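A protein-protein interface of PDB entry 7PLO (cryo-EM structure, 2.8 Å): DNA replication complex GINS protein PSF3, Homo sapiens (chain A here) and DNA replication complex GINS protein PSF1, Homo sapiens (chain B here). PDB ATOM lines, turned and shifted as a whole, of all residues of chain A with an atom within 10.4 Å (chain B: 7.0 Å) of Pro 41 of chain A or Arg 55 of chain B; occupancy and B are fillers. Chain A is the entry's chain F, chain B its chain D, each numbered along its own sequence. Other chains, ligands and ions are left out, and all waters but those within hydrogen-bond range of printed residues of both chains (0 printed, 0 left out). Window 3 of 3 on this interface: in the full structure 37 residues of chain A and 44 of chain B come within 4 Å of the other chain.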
ATOM      1  N   THR A  36       8.330  -5.588 -11.953  1.00  0.00           N
ATOM      2  CA  THR A  36       9.372  -4.801 -12.598  1.00  0.00           C
ATOM      3  C   THR A  36       8.780  -3.517 -13.167  1.00  0.00           C
ATOM      4  O   THR A  36       7.814  -3.559 -13.935  1.00  0.00           O
ATOM      5  CB  THR A  36      10.042  -5.603 -13.714  1.00  0.00           C
ATOM      6  OG1 THR A  36       9.058  -6.009 -14.673  1.00  0.00           O
ATOM      7  CG2 THR A  36      10.742  -6.834 -13.158  1.00  0.00           C
ATOM      8  N   THR A  38      10.860  -1.331 -14.852  1.00  0.00           N
ATOM      9  CA  THR A  38      11.628  -1.071 -16.062  1.00  0.00           C
ATOM     10  C   THR A  38      12.131  -2.394 -16.621  1.00  0.00           C
ATOM     11  O   THR A  38      12.317  -3.366 -15.886  1.00  0.00           O
ATOM     12  CB  THR A  38      12.821  -0.133 -15.807  1.00  0.00           C
ATOM     13  OG1 THR A  38      13.521  -0.545 -14.627  1.00  0.00           O
ATOM     14  CG2 THR A  38      12.356   1.311 -15.654  1.00  0.00           C
ATOM     15  N   ALA A  39      12.353  -2.420 -17.933  1.00  0.00           N
ATOM     16  CA  ALA A  39      12.811  -3.628 -18.604  1.00  0.00           C
ATOM     17  C   ALA A  39      14.296  -3.860 -18.346  1.00  0.00           C
ATOM     18  O   ALA A  39      15.079  -2.916 -18.208  1.00  0.00           O
ATOM     19  CB  ALA A  39      12.546  -3.538 -20.106  1.00  0.00           C
ATOM     20  N   MET A  40      14.675  -5.137 -18.297  1.00  0.00           N
ATOM     21  CA  MET A  40      16.004  -5.574 -17.860  1.00  0.00           C
ATOM     22  C   MET A  40      16.664  -6.420 -18.951  1.00  0.00           C
ATOM     23  O   MET A  40      16.369  -7.624 -19.058  1.00  0.00           O
ATOM     24  CB  MET A  40      15.884  -6.364 -16.556  1.00  0.00           C
ATOM     25  CG  MET A  40      15.080  -5.626 -15.481  1.00  0.00           C
ATOM     26  SD  MET A  40      15.155  -6.362 -13.836  1.00  0.00           S
ATOM     27  CE  MET A  40      16.754  -5.789 -13.271  1.00  0.00           C
ATOM     28  N   PRO A  41      17.539  -5.851 -19.795  1.00  0.00           N
ATOM     29  CA  PRO A  41      18.127  -6.644 -20.886  1.00  0.00           C
ATOM     30  C   PRO A  41      18.999  -7.795 -20.404  1.00  0.00           C
ATOM     31  O   PRO A  41      19.667  -7.714 -19.372  1.00  0.00           O
ATOM     32  CB  PRO A  41      18.958  -5.617 -21.665  1.00  0.00           C
ATOM     33  CG  PRO A  41      18.345  -4.322 -21.352  1.00  0.00           C
ATOM     34  CD  PRO A  41      17.890  -4.425 -19.938  1.00  0.00           C
ATOM     35  N   ARG A  42      18.952  -8.888 -21.173  1.00  0.00           N
ATOM     36  CA  ARG A  42      19.712 -10.123 -20.967  1.00  0.00           C
ATOM     37  C   ARG A  42      19.223 -10.964 -19.790  1.00  0.00           C
ATOM     38  O   ARG A  42      19.697 -12.088 -19.601  1.00  0.00           O
ATOM     39  CB  ARG A  42      21.205  -9.848 -20.755  1.00  0.00           C
ATOM     40  CG  ARG A  42      21.874  -8.905 -21.747  1.00  0.00           C
ATOM     41  CD  ARG A  42      23.364  -9.239 -21.869  1.00  0.00           C
ATOM     42  NE  ARG A  42      24.225  -8.077 -22.056  1.00  0.00           N
ATOM     43  CZ  ARG A  42      24.427  -7.440 -23.203  1.00  0.00           C
ATOM     44  NH1 ARG A  42      23.744  -7.739 -24.298  1.00  0.00           N
ATOM     45  NH2 ARG A  42      25.341  -6.475 -23.254  1.00  0.00           N
ATOM     46  N   LEU A  43      18.276 -10.455 -19.002  1.00  0.00           N
ATOM     47  CA  LEU A  43      17.879 -11.120 -17.772  1.00  0.00           C
ATOM     48  C   LEU A  43      16.848 -12.221 -17.996  1.00  0.00           C
ATOM     49  O   LEU A  43      16.610 -13.021 -17.082  1.00  0.00           O
ATOM     50  CB  LEU A  43      17.340 -10.079 -16.792  1.00  0.00           C
ATOM     51  CG  LEU A  43      17.453 -10.398 -15.301  1.00  0.00           C
ATOM     52  CD1 LEU A  43      18.896 -10.278 -14.822  1.00  0.00           C
ATOM     53  CD2 LEU A  43      16.554  -9.472 -14.511  1.00  0.00           C
ATOM     54  N   GLY A  44      16.267 -12.313 -19.195  1.00  0.00           N
ATOM     55  CA  GLY A  44      15.337 -13.388 -19.497  1.00  0.00           C
ATOM     56  C   GLY A  44      15.962 -14.767 -19.472  1.00  0.00           C
ATOM     57  O   GLY A  44      15.233 -15.763 -19.405  1.00  0.00           O
ATOM     58  N   ALA A  45      17.296 -14.850 -19.523  1.00  0.00           N
ATOM     59  CA  ALA A  45      17.977 -16.124 -19.328  1.00  0.00           C
ATOM     60  C   ALA A  45      17.668 -16.730 -17.964  1.00  0.00           C
ATOM     61  O   ALA A  45      17.722 -17.956 -17.811  1.00  0.00           O
ATOM     62  CB  ALA A  45      19.486 -15.937 -19.490  1.00  0.00           C
ATOM     63  N   PHE A  46      17.350 -15.893 -16.964  1.00  0.00           N
ATOM     64  CA  PHE A  46      17.080 -16.333 -15.601  1.00  0.00           C
ATOM     65  C   PHE A  46      15.671 -16.028 -15.120  1.00  0.00           C
ATOM     66  O   PHE A  46      15.123 -16.814 -14.342  1.00  0.00           O
ATOM     67  CB  PHE A  46      18.078 -15.676 -14.635  1.00  0.00           C
ATOM     68  CG  PHE A  46      19.471 -15.584 -15.184  1.00  0.00           C
ATOM     69  CD1 PHE A  46      20.265 -16.713 -15.286  1.00  0.00           C
ATOM     70  CD2 PHE A  46      19.984 -14.369 -15.607  1.00  0.00           C
ATOM     71  CE1 PHE A  46      21.545 -16.633 -15.796  1.00  0.00           C
ATOM     72  CE2 PHE A  46      21.265 -14.282 -16.117  1.00  0.00           C
ATOM     73  CZ  PHE A  46      22.047 -15.416 -16.211  1.00  0.00           C
ATOM     74  N   PHE A  47      15.065 -14.932 -15.576  1.00  0.00           N
ATOM     75  CA  PHE A  47      13.801 -14.426 -15.031  1.00  0.00           C
ATOM     76  C   PHE A  47      13.888 -14.257 -13.517  1.00  0.00           C
ATOM     77  O   PHE A  47      14.773 -13.567 -13.010  1.00  0.00           O
ATOM     78  CB  PHE A  47      12.623 -15.345 -15.385  1.00  0.00           C
ATOM     79  CG  PHE A  47      12.081 -15.136 -16.773  1.00  0.00           C
ATOM     80  CD1 PHE A  47      11.140 -14.149 -17.024  1.00  0.00           C
ATOM     81  CD2 PHE A  47      12.501 -15.935 -17.823  1.00  0.00           C
ATOM     82  CE1 PHE A  47      10.636 -13.958 -18.298  1.00  0.00           C
ATOM     83  CE2 PHE A  47      12.000 -15.749 -19.099  1.00  0.00           C
ATOM     84  CZ  PHE A  47      11.067 -14.760 -19.335  1.00  0.00           C
ATOM     85  N   ASN A  58      17.435 -12.366 -24.289  1.00  0.00           N
ATOM     86  CA  ASN A  58      16.166 -11.647 -24.253  1.00  0.00           C
ATOM     87  C   ASN A  58      15.944 -10.964 -22.902  1.00  0.00           C
ATOM     88  O   ASN A  58      16.405 -11.435 -21.862  1.00  0.00           O
ATOM     89  CB  ASN A  58      15.001 -12.600 -24.568  1.00  0.00           C
ATOM     90  CG  ASN A  58      14.918 -12.969 -26.052  1.00  0.00           C
ATOM     91  OD1 ASN A  58      15.404 -12.235 -26.912  1.00  0.00           O
ATOM     92  ND2 ASN A  58      14.292 -14.106 -26.353  1.00  0.00           N
ATOM     93  N   ALA A  59      15.231  -9.842 -22.948  1.00  0.00           N
ATOM     94  CA  ALA A  59      14.990  -9.012 -21.778  1.00  0.00           C
ATOM     95  C   ALA A  59      13.786  -9.509 -20.987  1.00  0.00           C
ATOM     96  O   ALA A  59      12.877 -10.142 -21.530  1.00  0.00           O
ATOM     97  CB  ALA A  59      14.747  -7.564 -22.203  1.00  0.00           C
ATOM     98  N   VAL A  60      13.789  -9.213 -19.691  1.00  0.00           N
ATOM     99  CA  VAL A  60      12.593  -9.362 -18.863  1.00  0.00           C
ATOM    100  C   VAL A  60      11.722  -8.139 -19.153  1.00  0.00           C
ATOM    101  O   VAL A  60      12.195  -7.009 -18.958  1.00  0.00           O
ATOM    102  CB  VAL A  60      12.946  -9.482 -17.370  1.00  0.00           C
ATOM    103  CG1 VAL A  60      11.716  -9.224 -16.481  1.00  0.00           C
ATOM    104  CG2 VAL A  60      13.551 -10.860 -17.076  1.00  0.00           C
ATOM    105  N   PRO A  61      10.475  -8.280 -19.613  1.00  0.00           N
ATOM    106  CA  PRO A  61       9.718  -7.093 -20.020  1.00  0.00           C
ATOM    107  C   PRO A  61       9.294  -6.243 -18.832  1.00  0.00           C
ATOM    108  O   PRO A  61       9.280  -6.681 -17.680  1.00  0.00           O
ATOM    109  CB  PRO A  61       8.502  -7.677 -20.741  1.00  0.00           C
ATOM    110  CG  PRO A  61       8.292  -8.979 -20.097  1.00  0.00           C
ATOM    111  CD  PRO A  61       9.662  -9.502 -19.783  1.00  0.00           C
ATOM    112  N   GLN A  62       8.947  -4.997 -19.141  1.00  0.00           N
ATOM    113  CA  GLN A  62       8.460  -4.073 -18.130  1.00  0.00           C
ATOM    114  C   GLN A  62       7.092  -4.514 -17.623  1.00  0.00           C
ATOM    115  O   GLN A  62       6.270  -5.050 -18.371  1.00  0.00           O
ATOM    116  CB  GLN A  62       8.386  -2.657 -18.708  1.00  0.00           C
ATOM    117  CG  GLN A  62       8.244  -1.538 -17.673  1.00  0.00           C
ATOM    118  CD  GLN A  62       6.802  -1.221 -17.290  1.00  0.00           C
ATOM    119  OE1 GLN A  62       5.854  -1.804 -17.816  1.00  0.00           O
ATOM    120  NE2 GLN A  62       6.639  -0.282 -16.367  1.00  0.00           N
ATOM    121  N   ILE A  83      13.550   0.433 -10.501  1.00  0.00           N
ATOM    122  CA  ILE A  83      13.788  -0.917 -11.002  1.00  0.00           C
ATOM    123  C   ILE A  83      12.549  -1.782 -10.816  1.00  0.00           C
ATOM    124  O   ILE A  83      12.093  -2.445 -11.755  1.00  0.00           O
ATOM    125  CB  ILE A  83      15.017  -1.550 -10.313  1.00  0.00           C
ATOM    126  CG1 ILE A  83      16.231  -0.603 -10.303  1.00  0.00           C
ATOM    127  CG2 ILE A  83      15.390  -2.874 -10.994  1.00  0.00           C
ATOM    128  CD1 ILE A  83      16.705  -0.125 -11.673  1.00  0.00           C
ATOM    129  N   ASP B  46      29.119  -5.414 -20.090  1.00  0.00           N
ATOM    130  CA  ASP B  46      27.886  -4.641 -20.189  1.00  0.00           C
ATOM    131  C   ASP B  46      28.111  -3.167 -19.869  1.00  0.00           C
ATOM    132  O   ASP B  46      27.517  -2.299 -20.514  1.00  0.00           O
ATOM    133  CB  ASP B  46      26.824  -5.236 -19.270  1.00  0.00           C
ATOM    134  CG  ASP B  46      26.326  -6.580 -19.754  1.00  0.00           C
ATOM    135  OD1 ASP B  46      26.865  -7.095 -20.756  1.00  0.00           O
ATOM    136  OD2 ASP B  46      25.385  -7.121 -19.139  1.00  0.00           O
ATOM    137  N   VAL B  47      28.952  -2.853 -18.877  1.00  0.00           N
ATOM    138  CA  VAL B  47      29.186  -1.450 -18.547  1.00  0.00           C
ATOM    139  C   VAL B  47      29.990  -0.776 -19.652  1.00  0.00           C
ATOM    140  O   VAL B  47      29.760   0.399 -19.970  1.00  0.00           O
ATOM    141  CB  VAL B  47      29.856  -1.309 -17.160  1.00  0.00           C
ATOM    142  CG1 VAL B  47      31.321  -1.737 -17.169  1.00  0.00           C
ATOM    143  CG2 VAL B  47      29.725   0.123 -16.629  1.00  0.00           C
ATOM    144  N   GLU B  49      29.734  -1.587 -22.815  1.00  0.00           N
ATOM    145  CA  GLU B  49      28.733  -1.352 -23.852  1.00  0.00           C
ATOM    146  C   GLU B  49      27.862  -0.147 -23.516  1.00  0.00           C
ATOM    147  O   GLU B  49      27.605   0.701 -24.378  1.00  0.00           O
ATOM    148  CB  GLU B  49      27.871  -2.604 -24.036  1.00  0.00           C
ATOM    149  CG  GLU B  49      26.809  -2.494 -25.133  1.00  0.00           C
ATOM    150  CD  GLU B  49      26.087  -3.805 -25.390  1.00  0.00           C
ATOM    151  OE1 GLU B  49      26.628  -4.873 -25.035  1.00  0.00           O
ATOM    152  OE2 GLU B  49      24.970  -3.765 -25.946  1.00  0.00           O
ATOM    153  N   ALA B  50      27.424  -0.038 -22.261  1.00  0.00           N
ATOM    154  CA  ALA B  50      26.512   1.036 -21.881  1.00  0.00           C
ATOM    155  C   ALA B  50      27.188   2.398 -21.964  1.00  0.00           C
ATOM    156  O   ALA B  50      26.566   3.377 -22.392  1.00  0.00           O
ATOM    157  CB  ALA B  50      25.975   0.792 -20.471  1.00  0.00           C
ATOM    158  N   LYS B  51      28.458   2.483 -21.564  1.00  0.00           N
ATOM    159  CA  LYS B  51      29.152   3.766 -21.586  1.00  0.00           C
ATOM    160  C   LYS B  51      29.614   4.128 -22.994  1.00  0.00           C
ATOM    161  O   LYS B  51      29.242   5.180 -23.525  1.00  0.00           O
ATOM    162  CB  LYS B  51      30.337   3.738 -20.619  1.00  0.00           C
ATOM    163  CG  LYS B  51      29.925   3.797 -19.158  1.00  0.00           C
ATOM    164  CD  LYS B  51      31.129   3.903 -18.241  1.00  0.00           C
ATOM    165  CE  LYS B  51      30.704   4.036 -16.789  1.00  0.00           C
ATOM    166  NZ  LYS B  51      31.871   4.177 -15.876  1.00  0.00           N
ATOM    167  N   SER B  52      30.436   3.273 -23.613  1.00  0.00           N
ATOM    168  CA  SER B  52      30.983   3.604 -24.925  1.00  0.00           C
ATOM    169  C   SER B  52      29.891   3.658 -25.988  1.00  0.00           C
ATOM    170  O   SER B  52      29.895   4.555 -26.840  1.00  0.00           O
ATOM    171  CB  SER B  52      32.059   2.591 -25.313  1.00  0.00           C
ATOM    172  OG  SER B  52      31.503   1.303 -25.509  1.00  0.00           O
ATOM    173  N   GLY B  53      28.951   2.712 -25.960  1.00  0.00           N
ATOM    174  CA  GLY B  53      27.850   2.713 -26.904  1.00  0.00           C
ATOM    175  C   GLY B  53      26.693   3.621 -26.545  1.00  0.00           C
ATOM    176  O   GLY B  53      25.790   3.797 -27.368  1.00  0.00           O
ATOM    177  N   GLY B  54      26.690   4.194 -25.342  1.00  0.00           N
ATOM    178  CA  GLY B  54      25.586   5.033 -24.918  1.00  0.00           C
ATOM    179  C   GLY B  54      24.288   4.302 -24.666  1.00  0.00           C
ATOM    180  O   GLY B  54      23.247   4.951 -24.530  1.00  0.00           O
ATOM    181  N   ARG B  55      24.314   2.973 -24.590  1.00  0.00           N
ATOM    182  CA  ARG B  55      23.102   2.188 -24.398  1.00  0.00           C
ATOM    183  C   ARG B  55      22.688   2.252 -22.932  1.00  0.00           C
ATOM    184  O   ARG B  55      23.408   1.764 -22.054  1.00  0.00           O
ATOM    185  CB  ARG B  55      23.336   0.747 -24.847  1.00  0.00           C
ATOM    186  CG  ARG B  55      22.132  -0.149 -24.668  1.00  0.00           C
ATOM    187  CD  ARG B  55      22.277  -1.493 -25.356  1.00  0.00           C
ATOM    188  NE  ARG B  55      21.071  -2.292 -25.165  1.00  0.00           N
ATOM    189  CZ  ARG B  55      20.953  -3.586 -25.440  1.00  0.00           C
ATOM    190  NH1 ARG B  55      21.961  -4.292 -25.932  1.00  0.00           N
ATOM    191  NH2 ARG B  55      19.791  -4.190 -25.210  1.00  0.00           N
ATOM    192  N   SER B  56      21.523   2.843 -22.667  1.00  0.00           N
ATOM    193  CA  SER B  56      21.113   3.148 -21.301  1.00  0.00           C
ATOM    194  C   SER B  56      20.344   2.019 -20.625  1.00  0.00           C
ATOM    195  O   SER B  56      20.377   1.918 -19.394  1.00  0.00           O
ATOM    196  CB  SER B  56      20.253   4.414 -21.286  1.00  0.00           C
ATOM    197  OG  SER B  56      19.886   4.762 -19.962  1.00  0.00           O
ATOM    198  N   ASP B  57      19.652   1.166 -21.384  1.00  0.00           N
ATOM    199  CA  ASP B  57      18.750   0.201 -20.760  1.00  0.00           C
ATOM    200  C   ASP B  57      19.475  -0.926 -20.029  1.00  0.00           C
ATOM    201  O   ASP B  57      18.824  -1.661 -19.280  1.00  0.00           O
ATOM    202  CB  ASP B  57      17.797  -0.385 -21.808  1.00  0.00           C
ATOM    203  CG  ASP B  57      18.511  -1.205 -22.859  1.00  0.00           C
ATOM    204  OD1 ASP B  57      19.696  -0.933 -23.116  1.00  0.00           O
ATOM    205  OD2 ASP B  57      17.883  -2.121 -23.431  1.00  0.00           O
ATOM    206  N   LEU B  58      20.791  -1.081 -20.206  1.00  0.00           N
ATOM    207  CA  LEU B  58      21.539  -2.117 -19.497  1.00  0.00           C
ATOM    208  C   LEU B  58      21.731  -1.820 -18.010  1.00  0.00           C
ATOM    209  O   LEU B  58      22.111  -2.733 -17.266  1.00  0.00           O
ATOM    210  CB  LEU B  58      22.909  -2.305 -20.153  1.00  0.00           C
ATOM    211  CG  LEU B  58      22.942  -3.074 -21.476  1.00  0.00           C
ATOM    212  CD1 LEU B  58      24.219  -2.769 -22.243  1.00  0.00           C
ATOM    213  CD2 LEU B  58      22.822  -4.570 -21.227  1.00  0.00           C
ATOM    214  N   ILE B  59      21.463  -0.578 -17.579  1.00  0.00           N
ATOM    215  CA  ILE B  59      21.759  -0.178 -16.194  1.00  0.00           C
ATOM    216  C   ILE B  59      21.065  -1.055 -15.159  1.00  0.00           C
ATOM    217  O   ILE B  59      21.701  -1.395 -14.142  1.00  0.00           O
ATOM    218  CB  ILE B  59      21.455   1.316 -16.008  1.00  0.00           C
ATOM    219  CG1 ILE B  59      22.425   2.179 -16.835  1.00  0.00           C
ATOM    220  CG2 ILE B  59      21.526   1.716 -14.528  1.00  0.00           C
ATOM    221  CD1 ILE B  59      21.930   3.595 -17.118  1.00  0.00           C
ATOM    222  N   PRO B  60      19.776  -1.408 -15.294  1.00  0.00           N
ATOM    223  CA  PRO B  60      19.190  -2.357 -14.327  1.00  0.00           C
ATOM    224  C   PRO B  60      19.915  -3.692 -14.244  1.00  0.00           C
ATOM    225  O   PRO B  60      20.074  -4.233 -13.144  1.00  0.00           O
ATOM    226  CB  PRO B  60      17.745  -2.524 -14.832  1.00  0.00           C
ATOM    227  CG  PRO B  60      17.678  -1.816 -16.149  1.00  0.00           C
ATOM    228  CD  PRO B  60      18.713  -0.758 -16.081  1.00  0.00           C
ATOM    229  N   THR B  61      20.384  -4.231 -15.370  1.00  0.00           N
ATOM    230  CA  THR B  61      21.127  -5.487 -15.321  1.00  0.00           C
ATOM    231  C   THR B  61      22.488  -5.305 -14.656  1.00  0.00           C
ATOM    232  O   THR B  61      22.965  -6.217 -13.958  1.00  0.00           O
ATOM    233  CB  THR B  61      21.287  -6.053 -16.731  1.00  0.00           C
ATOM    234  OG1 THR B  61      20.035  -5.965 -17.423  1.00  0.00           O
ATOM    235  CG2 THR B  61      21.722  -7.512 -16.682  1.00  0.00           C
ATOM    236  N   ILE B  62      23.125  -4.145 -14.865  1.00  0.00           N
ATOM    237  CA  ILE B  62      24.365  -3.834 -14.154  1.00  0.00           C
ATOM    238  C   ILE B  62      24.129  -3.888 -12.650  1.00  0.00           C
ATOM    239  O   ILE B  62      24.886  -4.526 -11.902  1.00  0.00           O
ATOM    240  CB  ILE B  62      24.904  -2.450 -14.575  1.00  0.00           C
ATOM    241  CG1 ILE B  62      25.249  -2.392 -16.072  1.00  0.00           C
ATOM    242  CG2 ILE B  62      26.123  -2.050 -13.729  1.00  0.00           C
ATOM    243  CD1 ILE B  62      26.329  -3.342 -16.548  1.00  0.00           C
ATOM    244  N   ARG B  65      23.618  -7.596 -11.373  1.00  0.00           N
ATOM    245  CA  ARG B  65      24.821  -8.401 -11.174  1.00  0.00           C
ATOM    246  C   ARG B  65      25.687  -7.854 -10.047  1.00  0.00           C
ATOM    247  O   ARG B  65      26.330  -8.634  -9.335  1.00  0.00           O
ATOM    248  CB  ARG B  65      25.641  -8.476 -12.453  1.00  0.00           C
ATOM    249  CG  ARG B  65      25.022  -9.296 -13.561  1.00  0.00           C
ATOM    250  CD  ARG B  65      26.077  -9.662 -14.586  1.00  0.00           C
ATOM    251  NE  ARG B  65      25.502  -9.928 -15.900  1.00  0.00           N
ATOM    252  CZ  ARG B  65      25.215  -9.008 -16.813  1.00  0.00           C
ATOM    253  NH1 ARG B  65      25.415  -7.716 -16.596  1.00  0.00           N
ATOM    254  NH2 ARG B  65      24.709  -9.393 -17.981  1.00  0.00           N
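The side-chain carboxylate of Asp 46 of chain B is in salt-bridge range of the guanidinium group of Arg 42 of chain A. OE1 of Glu 49 of chain B is in salt-bridge range of NH2 of Arg 42 of chain A (2.7 Å). The side-chain hydroxyl (OG1) of Thr 61 of chain B sits at hydrogen-bond distance from the backbone carbonyl oxygen (O) of Pro 41 of chain A, 2.6 Å away.
OD2 of Asp 46 of chain B is in salt-bridge range of NH1 of Arg 65 of chain B, 2.6 Å away. The side-chain carboxylate (OE2) of Glu 49 of chain B is in salt-bridge range of the guanidinium group (NH1) of Arg 55 of chain B. N of Arg 55 of chain B is in hydrogen-bond range of O of Ala 50 of chain B. The side-chain carboxylate of Asp 57 of chain B lies within salt-bridge range of the guanidinium group of Arg 55 of chain B, 2.8 Å away. N of Val 60 of chain A lies within hydrogen-bond range of O of Met 40 of chain A, 3.1 Å away.
Among the printed residues, merely in contact across the chains: Ala 39 of chain A with Pro 60 of chain B (3.5 Å), Met 40 of chain A with Pro 60 of chain B (3.7 Å), Met 40 of chain A with Thr 61 of chain B (3.7 Å), Pro 41 of chain A with Arg 55 of chain B (3.9 Å), Pro 41 of chain A with Asp 57 of chain B (3.0 Å) and Arg 42 of chain A with Leu 58 of chain B (3.8 Å).
Arg 55 of chain B touches one residue of chain A. No residue of chain A comes within 4 Å of Ala 50 of chain B. No residue of chain A comes within 4 Å of Gly 53 of chain B. No residue of chain A comes within 4 Å of Gly 54 of chain B. No residue of chain A comes within 4 Å of Ser 56 of chain B. Printed residues of chain A within 4 Å of Asp 57 of chain B: Pro 41 (3.0 Å). Leu 58 of chain B touches just one residue of chain A: Arg 42 (3.8 Å). Of the printed residues of chain A, Glu 49 of chain B touches Arg 42. Of the printed residues of chain B, Arg 42 of chain A touches Asp 46, Glu 49 and Leu 58. Printed residues of chain A within 4 Å of Pro 60 of chain B: Ala 39 and Met 40. Thr 38 of chain A touches none of the printed residues of chain B. Ala 45 of chain A touches none of the printed residues of chain B. The nearest residue of chain B that does not touch Pro 41 of chain A is Leu 58 of chain B (4.03 Å). The nearest residue of chain A that does not touch Arg 55 of chain B is Arg 42 of chain A (4.2 Å). The nearest printed residue of chain A that does not touch Thr 61 of chain B is Leu 43 of chain A (4.4 Å).
Of the 17 printed residues of chain A, 4 touch a printed residue of chain B. Along chain A the printed residues that touch a printed residue of chain B span positions 39 to 42. Printed residues of chain B that touch a printed residue of chain A: Asp 46, Glu 49, Arg 55, Asp 57, Leu 58, Pro 60 and Thr 61. Among the printed residues, 9 pairs touch across the chains. Among the printed residues, Asp or Glu carboxylates within 4 Å of a Lys or Arg side-chain nitrogen of the other chain: Arg 42 of chain A with Asp 46 of chain B (3.0 Å) and Arg 42 of chain A with Glu 49 of chain B (2.7 Å).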
